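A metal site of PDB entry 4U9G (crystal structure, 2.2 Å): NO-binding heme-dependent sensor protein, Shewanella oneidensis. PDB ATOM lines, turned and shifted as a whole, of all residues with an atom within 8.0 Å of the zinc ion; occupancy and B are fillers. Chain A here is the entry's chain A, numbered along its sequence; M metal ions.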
ATOM      1  N   TYR A 132     -21.615  -4.215  15.197  1.00  0.00           N
ATOM      2  CA  TYR A 132     -20.952  -3.760  16.414  1.00  0.00           C
ATOM      3  C   TYR A 132     -21.315  -4.626  17.602  1.00  0.00           C
ATOM      4  O   TYR A 132     -22.469  -5.037  17.761  1.00  0.00           O
ATOM      5  CB  TYR A 132     -21.312  -2.290  16.682  1.00  0.00           C
ATOM      6  CG  TYR A 132     -20.948  -1.786  18.074  1.00  0.00           C
ATOM      7  CD1 TYR A 132     -21.791  -2.013  19.151  1.00  0.00           C
ATOM      8  CD2 TYR A 132     -19.783  -1.077  18.302  1.00  0.00           C
ATOM      9  CE1 TYR A 132     -21.471  -1.567  20.420  1.00  0.00           C
ATOM     10  CE2 TYR A 132     -19.454  -0.614  19.562  1.00  0.00           C
ATOM     11  CZ  TYR A 132     -20.309  -0.863  20.619  1.00  0.00           C
ATOM     12  OH  TYR A 132     -19.995  -0.418  21.873  1.00  0.00           O
ATOM     13  N   ARG A 137     -21.735  -1.460  25.289  1.00  0.00           N
ATOM     14  CA  ARG A 137     -22.949  -1.070  24.557  1.00  0.00           C
ATOM     15  C   ARG A 137     -22.946   0.415  24.170  1.00  0.00           C
ATOM     16  O   ARG A 137     -23.912   1.143  24.426  1.00  0.00           O
ATOM     17  CB  ARG A 137     -24.180  -1.403  25.400  1.00  0.00           C
ATOM     18  CG  ARG A 137     -24.232  -2.853  25.833  1.00  0.00           C
ATOM     19  CD  ARG A 137     -25.661  -3.322  26.091  1.00  0.00           C
ATOM     20  NE  ARG A 137     -26.243  -2.665  27.256  1.00  0.00           N
ATOM     21  CZ  ARG A 137     -27.460  -2.898  27.704  1.00  0.00           C
ATOM     22  NH1 ARG A 137     -28.244  -3.766  27.087  1.00  0.00           N
ATOM     23  NH2 ARG A 137     -27.915  -2.253  28.777  1.00  0.00           N
ATOM     24  N   LEU A 138     -21.866   0.837  23.529  1.00  0.00           N
ATOM     25  CA  LEU A 138     -21.690   2.228  23.129  1.00  0.00           C
ATOM     26  C   LEU A 138     -21.939   2.408  21.641  1.00  0.00           C
ATOM     27  O   LEU A 138     -21.227   3.162  20.972  1.00  0.00           O
ATOM     28  CB  LEU A 138     -20.291   2.703  23.512  1.00  0.00           C
ATOM     29  CG  LEU A 138     -20.078   2.864  25.016  1.00  0.00           C
ATOM     30  CD1 LEU A 138     -18.599   2.999  25.356  1.00  0.00           C
ATOM     31  CD2 LEU A 138     -20.839   4.082  25.533  1.00  0.00           C
ATOM     32  N   CYS A 139     -22.960   1.729  21.122  1.00  0.00           N
ATOM     33  CA  CYS A 139     -23.288   1.776  19.705  1.00  0.00           C
ATOM     34  C   CYS A 139     -23.633   3.180  19.223  1.00  0.00           C
ATOM     35  O   CYS A 139     -23.399   3.524  18.066  1.00  0.00           O
ATOM     36  CB  CYS A 139     -24.455   0.828  19.384  1.00  0.00           C
ATOM     37  SG  CYS A 139     -25.939   1.101  20.386  1.00  0.00           S
ATOM     38  N   PHE A 140     -24.185   4.006  20.107  1.00  0.00           N
ATOM     39  CA  PHE A 140     -24.534   5.369  19.727  1.00  0.00           C
ATOM     40  C   PHE A 140     -23.298   6.255  19.689  1.00  0.00           C
ATOM     41  O   PHE A 140     -23.260   7.238  18.946  1.00  0.00           O
ATOM     42  CB  PHE A 140     -25.572   5.936  20.682  1.00  0.00           C
ATOM     43  CG  PHE A 140     -26.952   5.381  20.455  1.00  0.00           C
ATOM     44  CD1 PHE A 140     -27.737   5.866  19.434  1.00  0.00           C
ATOM     45  CD2 PHE A 140     -27.442   4.355  21.248  1.00  0.00           C
ATOM     46  CE1 PHE A 140     -29.001   5.358  19.207  1.00  0.00           C
ATOM     47  CE2 PHE A 140     -28.701   3.840  21.032  1.00  0.00           C
ATOM     48  CZ  PHE A 140     -29.490   4.340  20.006  1.00  0.00           C
ATOM     49  N   ALA A 142     -20.581   4.987  18.558  1.00  0.00           N
ATOM     50  CA  ALA A 142     -20.101   4.514  17.254  1.00  0.00           C
ATOM     51  C   ALA A 142     -20.779   5.275  16.122  1.00  0.00           C
ATOM     52  O   ALA A 142     -20.120   5.656  15.153  1.00  0.00           O
ATOM     53  CB  ALA A 142     -20.333   3.012  17.097  1.00  0.00           C
ATOM     54  N   GLU A 143     -22.077   5.500  16.248  1.00  0.00           N
ATOM     55  CA  GLU A 143     -22.819   6.282  15.260  1.00  0.00           C
ATOM     56  C   GLU A 143     -22.233   7.676  15.120  1.00  0.00           C
ATOM     57  O   GLU A 143     -21.949   8.125  14.015  1.00  0.00           O
ATOM     58  CB  GLU A 143     -24.309   6.381  15.629  1.00  0.00           C
ATOM     59  CG  GLU A 143     -25.212   5.473  14.835  1.00  0.00           C
ATOM     60  CD  GLU A 143     -26.686   5.837  14.960  1.00  0.00           C
ATOM     61  OE1 GLU A 143     -27.487   4.927  15.257  1.00  0.00           O
ATOM     62  OE2 GLU A 143     -27.034   7.015  14.753  1.00  0.00           O
ATOM     63  N   HIS A 161     -30.240   1.782  12.279  1.00  0.00           N
ATOM     64  CA  HIS A 161     -29.778   1.138  13.505  1.00  0.00           C
ATOM     65  C   HIS A 161     -30.939   0.352  14.130  1.00  0.00           C
ATOM     66  O   HIS A 161     -31.408   0.666  15.217  1.00  0.00           O
ATOM     67  CB  HIS A 161     -29.214   2.214  14.447  1.00  0.00           C
ATOM     68  CG  HIS A 161     -28.521   1.685  15.661  1.00  0.00           C
ATOM     69  ND1 HIS A 161     -27.711   2.474  16.450  1.00  0.00           N
ATOM     70  CD2 HIS A 161     -28.510   0.457  16.221  1.00  0.00           C
ATOM     71  CE1 HIS A 161     -27.230   1.750  17.447  1.00  0.00           C
ATOM     72  NE2 HIS A 161     -27.698   0.519  17.336  1.00  0.00           N
ATOM     73  N   ASP A 162     -31.389  -0.680  13.416  1.00  0.00           N
ATOM     74  CA  ASP A 162     -32.643  -1.362  13.732  1.00  0.00           C
ATOM     75  C   ASP A 162     -32.449  -2.682  14.477  1.00  0.00           C
ATOM     76  O   ASP A 162     -33.395  -3.227  15.028  1.00  0.00           O
ATOM     77  CB  ASP A 162     -33.449  -1.601  12.464  1.00  0.00           C
ATOM     78  CG  ASP A 162     -33.873  -0.301  11.788  1.00  0.00           C
ATOM     79  OD1 ASP A 162     -34.301   0.622  12.502  1.00  0.00           O
ATOM     80  OD2 ASP A 162     -33.773  -0.212  10.549  1.00  0.00           O
ATOM     81  N   THR A 163     -31.220  -3.208  14.457  1.00  0.00           N
ATOM     82  CA  THR A 163     -30.837  -4.277  15.375  1.00  0.00           C
ATOM     83  C   THR A 163     -29.920  -3.627  16.397  1.00  0.00           C
ATOM     84  O   THR A 163     -28.955  -2.952  16.010  1.00  0.00           O
ATOM     85  CB  THR A 163     -30.114  -5.448  14.661  1.00  0.00           C
ATOM     86  OG1 THR A 163     -30.948  -5.965  13.623  1.00  0.00           O
ATOM     87  CG2 THR A 163     -29.779  -6.564  15.641  1.00  0.00           C
ATOM     88  N   CYS A 164     -30.221  -3.806  17.679  1.00  0.00           N
ATOM     89  CA  CYS A 164     -29.491  -3.092  18.726  1.00  0.00           C
ATOM     90  C   CYS A 164     -29.448  -3.870  20.044  1.00  0.00           C
ATOM     91  O   CYS A 164     -30.409  -4.541  20.423  1.00  0.00           O
ATOM     92  CB  CYS A 164     -30.124  -1.714  18.958  1.00  0.00           C
ATOM     93  SG  CYS A 164     -29.257  -0.687  20.164  1.00  0.00           S
ATOM     94  N   MET A 165     -28.318  -3.757  20.734  1.00  0.00           N
ATOM     95  CA  MET A 165     -28.136  -4.419  22.016  1.00  0.00           C
ATOM     96  C   MET A 165     -29.087  -3.861  23.064  1.00  0.00           C
ATOM     97  O   MET A 165     -29.445  -4.546  24.028  1.00  0.00           O
ATOM     98  CB  MET A 165     -26.683  -4.266  22.481  1.00  0.00           C
ATOM     99  CG  MET A 165     -25.662  -4.910  21.535  1.00  0.00           C
ATOM    100  SD  MET A 165     -23.949  -4.844  22.127  1.00  0.00           S
ATOM    101  CE  MET A 165     -23.985  -6.088  23.420  1.00  0.00           C
ATOM    102  N   HIS A 166     -29.516  -2.619  22.864  1.00  0.00           N
ATOM    103  CA  HIS A 166     -30.429  -1.966  23.796  1.00  0.00           C
ATOM    104  C   HIS A 166     -31.880  -2.402  23.601  1.00  0.00           C
ATOM    105  O   HIS A 166     -32.715  -2.155  24.463  1.00  0.00           O
ATOM    106  CB  HIS A 166     -30.321  -0.447  23.653  1.00  0.00           C
ATOM    107  CG  HIS A 166     -29.026   0.098  24.149  1.00  0.00           C
ATOM    108  ND1 HIS A 166     -28.730   0.211  25.491  1.00  0.00           N
ATOM    109  CD2 HIS A 166     -27.936   0.566  23.490  1.00  0.00           C
ATOM    110  CE1 HIS A 166     -27.516   0.716  25.638  1.00  0.00           C
ATOM    111  NE2 HIS A 166     -27.019   0.941  24.438  1.00  0.00           N
ATOM    112  N   THR A 167     -32.176  -3.042  22.460  1.00  0.00           N
ATOM    113  CA  THR A 167     -33.494  -3.634  22.243  1.00  0.00           C
ATOM    114  C   THR A 167     -33.419  -5.172  22.256  1.00  0.00           C
ATOM    115  O   THR A 167     -34.285  -5.840  21.714  1.00  0.00           O
ATOM    116  CB  THR A 167     -34.136  -3.169  20.917  1.00  0.00           C
ATOM    117  OG1 THR A 167     -33.319  -3.563  19.804  1.00  0.00           O
ATOM    118  CG2 THR A 167     -34.333  -1.659  20.911  1.00  0.00           C
ATOM    119  N   ALA A 169     -30.794  -7.541  21.397  1.00  0.00           N
ATOM    120  CA  ALA A 169     -29.872  -8.357  20.603  1.00  0.00           C
ATOM    121  C   ALA A 169     -28.497  -8.419  21.283  1.00  0.00           C
ATOM    122  O   ALA A 169     -28.246  -7.683  22.227  1.00  0.00           O
ATOM    123  CB  ALA A 169     -29.748  -7.817  19.183  1.00  0.00           C
ATOM    124  N   HIS A 171     -25.827  -7.847  19.577  1.00  0.00           N
ATOM    125  CA  HIS A 171     -25.024  -6.987  18.712  1.00  0.00           C
ATOM    126  C   HIS A 171     -25.901  -5.904  18.113  1.00  0.00           C
ATOM    127  O   HIS A 171     -27.137  -5.963  18.205  1.00  0.00           O
ATOM    128  CB  HIS A 171     -24.353  -7.786  17.602  1.00  0.00           C
ATOM    129  CG  HIS A 171     -25.321  -8.336  16.600  1.00  0.00           C
ATOM    130  ND1 HIS A 171     -26.072  -9.462  16.834  1.00  0.00           N
ATOM    131  CD2 HIS A 171     -25.670  -7.892  15.367  1.00  0.00           C
ATOM    132  CE1 HIS A 171     -26.841  -9.699  15.779  1.00  0.00           C
ATOM    133  NE2 HIS A 171     -26.611  -8.767  14.879  1.00  0.00           N
ATOM    134  N   CYS A 172     -25.270  -4.909  17.492  1.00  0.00           N
ATOM    135  CA  CYS A 172     -25.980  -3.917  16.710  1.00  0.00           C
ATOM    136  C   CYS A 172     -25.583  -4.002  15.246  1.00  0.00           C
ATOM    137  O   CYS A 172     -24.436  -4.340  14.934  1.00  0.00           O
ATOM    138  CB  CYS A 172     -25.714  -2.500  17.232  1.00  0.00           C
ATOM    139  SG  CYS A 172     -25.941  -2.279  19.009  1.00  0.00           S
ATOM    140  N   MET A 173     -26.524  -3.717  14.356  1.00  0.00           N
ATOM    141  CA  MET A 173     -26.239  -3.565  12.934  1.00  0.00           C
ATOM    142  C   MET A 173     -26.451  -2.115  12.526  1.00  0.00           C
ATOM    143  O   MET A 173     -27.558  -1.586  12.614  1.00  0.00           O
ATOM    144  CB  MET A 173     -27.146  -4.473  12.086  1.00  0.00           C
ATOM    145  CG  MET A 173     -26.848  -5.962  12.172  1.00  0.00           C
ATOM    146  SD  MET A 173     -25.185  -6.443  11.643  1.00  0.00           S
ATOM    147  CE  MET A 173     -24.929  -5.447  10.180  1.00  0.00           C
ATOM    148  N   LEU A 174     -25.369  -1.471  12.094  1.00  0.00           N
ATOM    149  CA  LEU A 174     -25.435  -0.101  11.602  1.00  0.00           C
ATOM    150  C   LEU A 174     -25.315  -0.130  10.099  1.00  0.00           C
ATOM    151  O   LEU A 174     -24.257  -0.407   9.558  1.00  0.00           O
ATOM    152  CB  LEU A 174     -24.340   0.768  12.221  1.00  0.00           C
ATOM    153  CG  LEU A 174     -24.575   1.276  13.651  1.00  0.00           C
ATOM    154  CD1 LEU A 174     -24.951   0.166  14.610  1.00  0.00           C
ATOM    155  CD2 LEU A 174     -23.349   2.018  14.150  1.00  0.00           C
HETATM  156 ZN    ZN M   1     -27.219  -0.348  19.106  1.00  0.00          ZN
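ND1 of His 161 sits at hydrogen-bond distance from OE1 of Glu 143 (2.7 Å). The side-chain sulfur (SG) of Cys 164 lies close to the backbone NH (N) of His 166. The side-chain sulfur of Cys 172 lies close to the backbone NH of Met 165, at 3.3 Å. The side-chain hydroxyl of Thr 167 sits at hydrogen-bond distance from the backbone carbonyl oxygen of Cys 164. NH1 of Arg 137 lies within hydrogen-bond range of O of Met 165, 3.4 Å away. The backbone NH (N) of Ala 169 is in hydrogen-bond range of the backbone carbonyl oxygen (O) of Cys 164 (3.2 Å). The backbone carbonyl oxygen (O) of Tyr 132 sits at hydrogen-bond distance from the backbone NH (N) of Cys 172, 2.8 Å away.
Met 165 touches the zinc ion. Of the 19 residues printed, 5 come within 4 Å of the zinc ion. The nearest printed residue that does not touch the zinc ion is Thr 163 (4.4 Å).
The zinc ion is bound by NE2 of His 161, SG of Cys 172, SG of Cys 139 and SG of Cys 164. The zinc ion has four donor atoms within binding distance.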
